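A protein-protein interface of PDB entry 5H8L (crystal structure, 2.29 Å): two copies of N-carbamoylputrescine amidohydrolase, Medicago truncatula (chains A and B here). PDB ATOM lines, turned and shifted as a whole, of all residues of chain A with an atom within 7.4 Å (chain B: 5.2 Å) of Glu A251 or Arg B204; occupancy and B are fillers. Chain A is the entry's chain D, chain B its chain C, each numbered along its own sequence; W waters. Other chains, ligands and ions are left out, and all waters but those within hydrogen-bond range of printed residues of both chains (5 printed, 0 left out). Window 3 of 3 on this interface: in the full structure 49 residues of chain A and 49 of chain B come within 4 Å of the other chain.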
ATOM      1  N   ARG A 204      30.058   3.270 -15.804  1.00  0.00           N
ATOM      2  CA  ARG A 204      28.742   2.664 -15.818  1.00  0.00           C
ATOM      3  C   ARG A 204      27.657   3.514 -15.194  1.00  0.00           C
ATOM      4  O   ARG A 204      26.513   3.599 -15.708  1.00  0.00           O
ATOM      5  CB  ARG A 204      28.775   1.285 -15.181  1.00  0.00           C
ATOM      6  CG  ARG A 204      29.411   0.278 -16.098  1.00  0.00           C
ATOM      7  CD  ARG A 204      29.190  -1.150 -15.596  1.00  0.00           C
ATOM      8  NE  ARG A 204      29.937  -1.377 -14.372  1.00  0.00           N
ATOM      9  CZ  ARG A 204      31.154  -1.958 -14.319  1.00  0.00           C
ATOM     10  NH1 ARG A 204      31.702  -2.469 -15.422  1.00  0.00           N
ATOM     11  NH2 ARG A 204      31.754  -2.103 -13.175  1.00  0.00           N
ATOM     12  N   VAL A 205      27.981   4.185 -14.100  1.00  0.00           N
ATOM     13  CA  VAL A 205      26.932   4.979 -13.457  1.00  0.00           C
ATOM     14  C   VAL A 205      26.543   6.162 -14.359  1.00  0.00           C
ATOM     15  O   VAL A 205      25.368   6.466 -14.507  1.00  0.00           O
ATOM     16  CB  VAL A 205      27.388   5.435 -12.063  1.00  0.00           C
ATOM     17  CG1 VAL A 205      26.496   6.522 -11.486  1.00  0.00           C
ATOM     18  CG2 VAL A 205      27.457   4.244 -11.135  1.00  0.00           C
ATOM     19  N   MET A 206      27.550   6.833 -14.954  1.00  0.00           N
ATOM     20  CA  MET A 206      27.281   7.956 -15.832  1.00  0.00           C
ATOM     21  C   MET A 206      26.561   7.524 -17.098  1.00  0.00           C
ATOM     22  O   MET A 206      25.605   8.167 -17.540  1.00  0.00           O
ATOM     23  CB  MET A 206      28.533   8.823 -16.113  1.00  0.00           C
ATOM     24  CG  MET A 206      28.641   9.924 -15.053  1.00  0.00           C
ATOM     25  SD  MET A 206      30.100  10.982 -15.361  1.00  0.00           S
ATOM     26  CE  MET A 206      31.319   9.711 -14.986  1.00  0.00           C
ATOM     27  N   GLN A 207      27.003   6.440 -17.674  1.00  0.00           N
ATOM     28  CA  GLN A 207      26.324   5.927 -18.845  1.00  0.00           C
ATOM     29  C   GLN A 207      24.828   5.678 -18.513  1.00  0.00           C
ATOM     30  O   GLN A 207      23.965   5.828 -19.366  1.00  0.00           O
ATOM     31  CB  GLN A 207      26.994   4.659 -19.311  1.00  0.00           C
ATOM     32  CG  GLN A 207      28.356   4.862 -19.935  1.00  0.00           C
ATOM     33  CD  GLN A 207      28.956   3.549 -20.312  1.00  0.00           C
ATOM     34  OE1 GLN A 207      29.525   2.872 -19.479  1.00  0.00           O
ATOM     35  NE2 GLN A 207      28.740   3.136 -21.548  1.00  0.00           N
ATOM     36  N   GLY A 208      24.545   5.308 -17.271  1.00  0.00           N
ATOM     37  CA  GLY A 208      23.180   5.067 -16.895  1.00  0.00           C
ATOM     38  C   GLY A 208      22.312   6.312 -16.912  1.00  0.00           C
ATOM     39  O   GLY A 208      21.164   6.249 -17.330  1.00  0.00           O
ATOM     40  N   HIS A 209      22.863   7.425 -16.482  1.00  0.00           N
ATOM     41  CA  HIS A 209      22.184   8.709 -16.523  1.00  0.00           C
ATOM     42  C   HIS A 209      21.882   9.106 -17.948  1.00  0.00           C
ATOM     43  O   HIS A 209      20.789   9.625 -18.260  1.00  0.00           O
ATOM     44  CB  HIS A 209      23.075   9.877 -15.971  1.00  0.00           C
ATOM     45  CG  HIS A 209      23.596   9.685 -14.565  1.00  0.00           C
ATOM     46  ND1 HIS A 209      22.989   8.869 -13.637  1.00  0.00           N
ATOM     47  CD2 HIS A 209      24.676  10.211 -13.942  1.00  0.00           C
ATOM     48  CE1 HIS A 209      23.662   8.908 -12.498  1.00  0.00           C
ATOM     49  NE2 HIS A 209      24.699   9.701 -12.663  1.00  0.00           N
ATOM     50  N   ALA A 210      22.859   8.943 -18.812  1.00  0.00           N
ATOM     51  CA  ALA A 210      22.632   9.339 -20.187  1.00  0.00           C
ATOM     52  C   ALA A 210      21.501   8.509 -20.823  1.00  0.00           C
ATOM     53  O   ALA A 210      20.672   9.053 -21.527  1.00  0.00           O
ATOM     54  CB  ALA A 210      23.883   9.209 -20.999  1.00  0.00           C
ATOM     55  N   GLY A 211      21.449   7.216 -20.513  1.00  0.00           N
ATOM     56  CA  GLY A 211      20.448   6.366 -21.068  1.00  0.00           C
ATOM     57  C   GLY A 211      19.089   6.600 -20.465  1.00  0.00           C
ATOM     58  O   GLY A 211      18.105   6.502 -21.135  1.00  0.00           O
ATOM     59  N   ALA A 212      19.044   6.943 -19.201  1.00  0.00           N
ATOM     60  CA  ALA A 212      17.762   7.065 -18.524  1.00  0.00           C
ATOM     61  C   ALA A 212      17.072   8.395 -18.806  1.00  0.00           C
ATOM     62  O   ALA A 212      15.876   8.504 -18.683  1.00  0.00           O
ATOM     63  CB  ALA A 212      17.939   6.883 -17.053  1.00  0.00           C
ATOM     64  N   LEU A 217      26.142  13.149 -22.594  1.00  0.00           N
ATOM     65  CA  LEU A 217      26.832  13.449 -21.362  1.00  0.00           C
ATOM     66  C   LEU A 217      28.367  13.499 -21.610  1.00  0.00           C
ATOM     67  O   LEU A 217      28.929  12.657 -22.311  1.00  0.00           O
ATOM     68  CB  LEU A 217      26.496  12.352 -20.377  1.00  0.00           C
ATOM     69  CG  LEU A 217      27.075  12.367 -18.955  1.00  0.00           C
ATOM     70  CD1 LEU A 217      26.201  11.455 -18.119  1.00  0.00           C
ATOM     71  CD2 LEU A 217      28.515  11.860 -18.917  1.00  0.00           C
ATOM     72  N   PHE A 244      35.378  10.960 -21.228  1.00  0.00           N
ATOM     73  CA  PHE A 244      34.618  10.440 -22.311  1.00  0.00           C
ATOM     74  C   PHE A 244      33.408  11.262 -22.649  1.00  0.00           C
ATOM     75  O   PHE A 244      33.042  12.214 -21.925  1.00  0.00           O
ATOM     76  CB  PHE A 244      34.201   9.022 -21.989  1.00  0.00           C
ATOM     77  CG  PHE A 244      33.210   8.930 -20.860  1.00  0.00           C
ATOM     78  CD1 PHE A 244      33.644   8.884 -19.556  1.00  0.00           C
ATOM     79  CD2 PHE A 244      31.869   8.937 -21.111  1.00  0.00           C
ATOM     80  CE1 PHE A 244      32.746   8.825 -18.482  1.00  0.00           C
ATOM     81  CE2 PHE A 244      30.947   8.880 -20.056  1.00  0.00           C
ATOM     82  CZ  PHE A 244      31.387   8.841 -18.743  1.00  0.00           C
ATOM     83  N   ILE A 245      32.807  10.895 -23.788  1.00  0.00           N
ATOM     84  CA  ILE A 245      31.531  11.465 -24.233  1.00  0.00           C
ATOM     85  C   ILE A 245      30.555  10.309 -24.550  1.00  0.00           C
ATOM     86  O   ILE A 245      30.870   9.394 -25.333  1.00  0.00           O
ATOM     87  CB  ILE A 245      31.706  12.363 -25.497  1.00  0.00           C
ATOM     88  CG1 ILE A 245      32.733  13.487 -25.236  1.00  0.00           C
ATOM     89  CG2 ILE A 245      30.374  12.988 -25.878  1.00  0.00           C
ATOM     90  CD1 ILE A 245      33.036  14.372 -26.454  1.00  0.00           C
ATOM     91  N   ALA A 246      29.407  10.335 -23.900  1.00  0.00           N
ATOM     92  CA  ALA A 246      28.369   9.345 -24.130  1.00  0.00           C
ATOM     93  C   ALA A 246      27.187   9.960 -24.884  1.00  0.00           C
ATOM     94  O   ALA A 246      26.867  11.112 -24.710  1.00  0.00           O
ATOM     95  CB  ALA A 246      27.872   8.769 -22.801  1.00  0.00           C
ATOM     96  N   GLY A 247      26.546   9.135 -25.693  1.00  0.00           N
ATOM     97  CA  GLY A 247      25.348   9.490 -26.413  1.00  0.00           C
ATOM     98  C   GLY A 247      24.078   9.200 -25.645  1.00  0.00           C
ATOM     99  O   GLY A 247      24.114   8.795 -24.477  1.00  0.00           O
ATOM    100  N   PRO A 248      22.931   9.429 -26.292  1.00  0.00           N
ATOM    101  CA  PRO A 248      21.710   9.455 -25.513  1.00  0.00           C
ATOM    102  C   PRO A 248      21.172   8.083 -25.093  1.00  0.00           C
ATOM    103  O   PRO A 248      20.189   8.040 -24.347  1.00  0.00           O
ATOM    104  CB  PRO A 248      20.726  10.249 -26.401  1.00  0.00           C
ATOM    105  CG  PRO A 248      21.223  10.115 -27.779  1.00  0.00           C
ATOM    106  CD  PRO A 248      22.740   9.929 -27.674  1.00  0.00           C
ATOM    107  N   THR A 249      21.765   6.990 -25.574  1.00  0.00           N
ATOM    108  CA  THR A 249      21.411   5.645 -25.053  1.00  0.00           C
ATOM    109  C   THR A 249      22.516   5.113 -24.125  1.00  0.00           C
ATOM    110  O   THR A 249      22.556   3.933 -23.769  1.00  0.00           O
ATOM    111  CB  THR A 249      21.252   4.614 -26.167  1.00  0.00           C
ATOM    112  OG1 THR A 249      22.507   4.474 -26.855  1.00  0.00           O
ATOM    113  CG2 THR A 249      20.123   5.008 -27.105  1.00  0.00           C
ATOM    114  N   GLY A 250      23.415   5.992 -23.745  1.00  0.00           N
ATOM    115  CA  GLY A 250      24.527   5.587 -22.934  1.00  0.00           C
ATOM    116  C   GLY A 250      25.781   5.075 -23.637  1.00  0.00           C
ATOM    117  O   GLY A 250      26.743   4.790 -22.945  1.00  0.00           O
ATOM    118  N   GLU A 251      25.766   4.969 -24.977  1.00  0.00           N
ATOM    119  CA  GLU A 251      26.912   4.498 -25.727  1.00  0.00           C
ATOM    120  C   GLU A 251      28.092   5.462 -25.567  1.00  0.00           C
ATOM    121  O   GLU A 251      27.932   6.665 -25.630  1.00  0.00           O
ATOM    122  CB  GLU A 251      26.613   4.369 -27.234  1.00  0.00           C
ATOM    123  CG  GLU A 251      27.668   3.436 -27.855  1.00  0.00           C
ATOM    124  CD  GLU A 251      27.589   3.107 -29.348  1.00  0.00           C
ATOM    125  OE1 GLU A 251      28.561   3.424 -30.073  1.00  0.00           O
ATOM    126  OE2 GLU A 251      26.604   2.460 -29.782  1.00  0.00           O
ATOM    127  N   ILE A 252      29.293   4.944 -25.397  1.00  0.00           N
ATOM    128  CA  ILE A 252      30.462   5.808 -25.328  1.00  0.00           C
ATOM    129  C   ILE A 252      30.834   6.089 -26.765  1.00  0.00           C
ATOM    130  O   ILE A 252      31.163   5.172 -27.500  1.00  0.00           O
ATOM    131  CB  ILE A 252      31.658   5.079 -24.697  1.00  0.00           C
ATOM    132  CG1 ILE A 252      31.347   4.625 -23.266  1.00  0.00           C
ATOM    133  CG2 ILE A 252      32.894   5.955 -24.688  1.00  0.00           C
ATOM    134  CD1 ILE A 252      31.017   5.695 -22.317  1.00  0.00           C
ATOM    135  N   VAL A 253      30.772   7.340 -27.182  1.00  0.00           N
ATOM    136  CA  VAL A 253      31.136   7.667 -28.553  1.00  0.00           C
ATOM    137  C   VAL A 253      32.555   8.157 -28.672  1.00  0.00           C
ATOM    138  O   VAL A 253      33.133   8.077 -29.728  1.00  0.00           O
ATOM    139  CB  VAL A 253      30.159   8.652 -29.222  1.00  0.00           C
ATOM    140  CG1 VAL A 253      28.708   8.093 -29.167  1.00  0.00           C
ATOM    141  CG2 VAL A 253      30.152   9.967 -28.513  1.00  0.00           C
ATOM    142  N   SER A 254      33.140   8.642 -27.590  1.00  0.00           N
ATOM    143  CA  SER A 254      34.514   9.012 -27.646  1.00  0.00           C
ATOM    144  C   SER A 254      35.106   8.848 -26.263  1.00  0.00           C
ATOM    145  O   SER A 254      34.467   9.227 -25.277  1.00  0.00           O
ATOM    146  CB  SER A 254      34.609  10.439 -28.172  1.00  0.00           C
ATOM    147  OG  SER A 254      35.945  10.833 -28.315  1.00  0.00           O
ATOM    148  N   PHE A 268      26.340  16.308 -31.928  1.00  0.00           N
ATOM    149  CA  PHE A 268      25.004  15.789 -31.564  1.00  0.00           C
ATOM    150  C   PHE A 268      23.905  16.596 -32.239  1.00  0.00           C
ATOM    151  O   PHE A 268      23.963  17.826 -32.293  1.00  0.00           O
ATOM    152  CB  PHE A 268      24.774  15.816 -30.047  1.00  0.00           C
ATOM    153  CG  PHE A 268      25.609  14.824 -29.320  1.00  0.00           C
ATOM    154  CD1 PHE A 268      25.431  13.470 -29.544  1.00  0.00           C
ATOM    155  CD2 PHE A 268      26.663  15.233 -28.481  1.00  0.00           C
ATOM    156  CE1 PHE A 268      26.238  12.529 -28.915  1.00  0.00           C
ATOM    157  CE2 PHE A 268      27.467  14.290 -27.830  1.00  0.00           C
ATOM    158  CZ  PHE A 268      27.246  12.921 -28.051  1.00  0.00           C
ATOM    159  N   ASP B 200      21.094  -2.957 -25.803  1.00  0.00           N
ATOM    160  CA  ASP B 200      22.236  -2.374 -25.155  1.00  0.00           C
ATOM    161  C   ASP B 200      21.855  -1.196 -24.313  1.00  0.00           C
ATOM    162  O   ASP B 200      22.434  -1.021 -23.238  1.00  0.00           O
ATOM    163  CB  ASP B 200      23.284  -1.948 -26.127  1.00  0.00           C
ATOM    164  CG  ASP B 200      23.827  -3.119 -26.916  1.00  0.00           C
ATOM    165  OD1 ASP B 200      23.924  -4.254 -26.351  1.00  0.00           O
ATOM    166  OD2 ASP B 200      24.082  -2.935 -28.115  1.00  0.00           O
ATOM    167  N   HIS B 201      20.887  -0.404 -24.801  1.00  0.00           N
ATOM    168  CA  HIS B 201      20.362   0.730 -24.072  1.00  0.00           C
ATOM    169  C   HIS B 201      19.743   0.235 -22.778  1.00  0.00           C
ATOM    170  O   HIS B 201      20.005   0.781 -21.692  1.00  0.00           O
ATOM    171  CB  HIS B 201      19.356   1.474 -24.941  1.00  0.00           C
ATOM    172  CG  HIS B 201      18.796   2.735 -24.343  1.00  0.00           C
ATOM    173  ND1 HIS B 201      17.714   3.379 -24.894  1.00  0.00           N
ATOM    174  CD2 HIS B 201      19.126   3.444 -23.243  1.00  0.00           C
ATOM    175  CE1 HIS B 201      17.415   4.446 -24.167  1.00  0.00           C
ATOM    176  NE2 HIS B 201      18.257   4.511 -23.162  1.00  0.00           N
ATOM    177  N   TRP B 202      18.950  -0.820 -22.887  1.00  0.00           N
ATOM    178  CA  TRP B 202      18.270  -1.446 -21.729  1.00  0.00           C
ATOM    179  C   TRP B 202      19.273  -1.925 -20.655  1.00  0.00           C
ATOM    180  O   TRP B 202      19.102  -1.637 -19.475  1.00  0.00           O
ATOM    181  CB  TRP B 202      17.455  -2.596 -22.250  1.00  0.00           C
ATOM    182  CG  TRP B 202      16.804  -3.522 -21.311  1.00  0.00           C
ATOM    183  CD1 TRP B 202      15.643  -3.310 -20.621  1.00  0.00           C
ATOM    184  CD2 TRP B 202      17.127  -4.888 -21.119  1.00  0.00           C
ATOM    185  NE1 TRP B 202      15.247  -4.470 -19.957  1.00  0.00           N
ATOM    186  CE2 TRP B 202      16.156  -5.446 -20.250  1.00  0.00           C
ATOM    187  CE3 TRP B 202      18.149  -5.705 -21.581  1.00  0.00           C
ATOM    188  CZ2 TRP B 202      16.222  -6.731 -19.809  1.00  0.00           C
ATOM    189  CZ3 TRP B 202      18.190  -7.011 -21.145  1.00  0.00           C
ATOM    190  CH2 TRP B 202      17.228  -7.504 -20.278  1.00  0.00           C
ATOM    191  N   LYS B 203      20.329  -2.622 -21.057  1.00  0.00           N
ATOM    192  CA  LYS B 203      21.332  -3.080 -20.085  1.00  0.00           C
ATOM    193  C   LYS B 203      22.061  -1.943 -19.350  1.00  0.00           C
ATOM    194  O   LYS B 203      22.173  -1.960 -18.131  1.00  0.00           O
ATOM    195  CB  LYS B 203      22.364  -3.996 -20.750  1.00  0.00           C
ATOM    196  CG  LYS B 203      21.846  -5.407 -20.956  1.00  0.00           C
ATOM    197  CD  LYS B 203      22.901  -6.303 -21.624  1.00  0.00           C
ATOM    198  CE  LYS B 203      22.706  -6.407 -23.127  1.00  0.00           C
ATOM    199  NZ  LYS B 203      23.838  -7.084 -23.829  1.00  0.00           N
ATOM    200  N   ARG B 204      22.505  -0.954 -20.108  1.00  0.00           N
ATOM    201  CA  ARG B 204      23.211   0.183 -19.586  1.00  0.00           C
ATOM    202  C   ARG B 204      22.421   0.951 -18.530  1.00  0.00           C
ATOM    203  O   ARG B 204      22.952   1.327 -17.505  1.00  0.00           O
ATOM    204  CB  ARG B 204      23.624   1.103 -20.727  1.00  0.00           C
ATOM    205  CG  ARG B 204      24.850   0.627 -21.471  1.00  0.00           C
ATOM    206  CD  ARG B 204      25.405   1.673 -22.432  1.00  0.00           C
ATOM    207  NE  ARG B 204      24.497   1.967 -23.537  1.00  0.00           N
ATOM    208  CZ  ARG B 204      24.636   1.496 -24.771  1.00  0.00           C
ATOM    209  NH1 ARG B 204      25.671   0.723 -25.080  1.00  0.00           N
ATOM    210  NH2 ARG B 204      23.758   1.812 -25.696  1.00  0.00           N
ATOM    211  N   VAL B 205      21.129   1.141 -18.747  1.00  0.00           N
ATOM    212  CA  VAL B 205      20.336   1.855 -17.797  1.00  0.00           C
ATOM    213  C   VAL B 205      20.268   1.103 -16.475  1.00  0.00           C
ATOM    214  O   VAL B 205      20.471   1.702 -15.381  1.00  0.00           O
ATOM    215  CB  VAL B 205      18.953   2.115 -18.349  1.00  0.00           C
ATOM    216  CG1 VAL B 205      18.004   2.465 -17.213  1.00  0.00           C
ATOM    217  CG2 VAL B 205      19.050   3.216 -19.394  1.00  0.00           C
ATOM    218  N   MET B 206      20.049  -0.201 -16.574  1.00  0.00           N
ATOM    219  CA  MET B 206      19.959  -1.049 -15.392  1.00  0.00           C
ATOM    220  C   MET B 206      21.321  -1.264 -14.737  1.00  0.00           C
ATOM    221  O   MET B 206      21.462  -1.253 -13.507  1.00  0.00           O
ATOM    222  CB  MET B 206      19.344  -2.353 -15.782  1.00  0.00           C
ATOM    223  CG  MET B 206      17.803  -2.290 -15.705  1.00  0.00           C
ATOM    224  SD  MET B 206      17.178  -3.989 -15.762  1.00  0.00           S
ATOM    225  CE  MET B 206      17.450  -4.265 -17.529  1.00  0.00           C
ATOM    226  N   GLN B 207      22.359  -1.407 -15.556  1.00  0.00           N
ATOM    227  CA  GLN B 207      23.672  -1.437 -14.942  1.00  0.00           C
ATOM    228  C   GLN B 207      23.890  -0.149 -14.108  1.00  0.00           C
ATOM    229  O   GLN B 207      24.546  -0.182 -13.107  1.00  0.00           O
ATOM    230  CB  GLN B 207      24.729  -1.615 -15.976  1.00  0.00           C
ATOM    231  CG  GLN B 207      24.821  -3.008 -16.535  1.00  0.00           C
ATOM    232  CD  GLN B 207      25.819  -3.061 -17.659  1.00  0.00           C
ATOM    233  OE1 GLN B 207      25.491  -2.790 -18.795  1.00  0.00           O
ATOM    234  NE2 GLN B 207      27.056  -3.383 -17.336  1.00  0.00           N
ATOM    235  N   GLY B 208      23.277   0.956 -14.525  1.00  0.00           N
ATOM    236  CA  GLY B 208      23.468   2.226 -13.880  1.00  0.00           C
ATOM    237  C   GLY B 208      22.823   2.198 -12.517  1.00  0.00           C
ATOM    238  O   GLY B 208      23.366   2.748 -11.594  1.00  0.00           O
HETATM  239  O   HOH W   1      23.131   5.568 -12.945  1.00  0.00           O
HETATM  240  O   HOH W   2      22.342   1.819 -28.190  1.00  0.00           O
HETATM  241  O   HOH W   3      24.880   0.891 -28.598  1.00  0.00           O
HETATM  242  O   HOH W   4      20.351   4.554 -15.019  1.00  0.00           O
HETATM  243  O   HOH W   5      25.648   1.649 -17.492  1.00  0.00           O
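Printed residues of chain B that touch a printed residue of chain A: His B201, Arg B204, Val B205, Gln B207 and Gly B208.
Hydrophobic or aromatic side chains of chain B that line the printed part of chain A: His B201 and Val B205.
Arg A204 touches Gln B207, and with the chains exchanged Gln A207 touches Arg B204.
Arg A204 touches Gly B208, and with the chains exchanged Gly A208 touches Arg B204.
Positions printed for both chains: 204, 205, 206, 207 and 208.
Of the 11 pairs that touch across the chains among the printed residues, 4 have their exchanged pair printed and touching as well.
Of chain B, only Arg B204 (3.6 Å) comes within 4 Å of Glu A251.
Arg B204 touches just these residues of chain A: Gln A207 (3.7 Å), Gly A208 (3.8 Å), Thr A249 (2.8 Å), Gly A250 (3.4 Å) and Glu A251 (3.6 Å).
Printed residues of chain B within 4 Å of Arg A204: Gln B207 and Gly B208.
Printed residues of chain B within 4 Å of Gly A250: Arg B204 (3.4 Å).
Printed residues of chain B within 4 Å of Thr A249: His B201 and Arg B204.
Of the printed residues of chain A, His B201 touches Gly A211 and Thr A249.
The nearest residue of chain A that does not touch Arg B204 is Arg A204 (4.6 Å).
The backbone carbonyl oxygen (O) of Gly A211 sits at hydrogen-bond distance from a ring nitrogen (NE2) of His B201, at 2.8 Å.
NE of Arg B204 sits at hydrogen-bond distance from O of Thr A249 (2.8 Å).
Water W3 lies within hydrogen-bond range of the side-chain carboxylate of Glu A251 and the guanidinium group of Arg B204.
Water W5 bridges O of Arg B204 (2.7 Å) and O of Arg A204 (2.8 Å).
Water W2 lies within hydrogen-bond range of NH2 of Arg B204 (2.9 Å) and OG1 of Thr A249 (3.0 Å).
Water W1 lies within hydrogen-bond range of O of Val A205, O of Gly B208 and ND1 of His A209.
Water W4 lies within hydrogen-bond range of the backbone carbonyl oxygen of Val B205 (2.9 Å) and the backbone carbonyl oxygen of Gly A208 (3.0 Å).
The side-chain amide oxygen of Gln B207 sits close to the backbone carbonyl oxygen of Lys B203, 3.5 Å away.
The side-chain amide nitrogen (NE2) of Gln A207 is in hydrogen-bond range of the backbone carbonyl oxygen (O) of Gly A250 (2.9 Å).
Among the printed residues, merely in contact across the chains: Arg A204 with Gln B207, Arg A204 with Gly B208, Gln A207 with Arg B204, Gly A208 with Arg B204, Gly A211 with Val B205, Ala A212 with Val B205, Thr A249 with His B201, Gly A250 with Arg B204 and Glu A251 with Arg B204.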
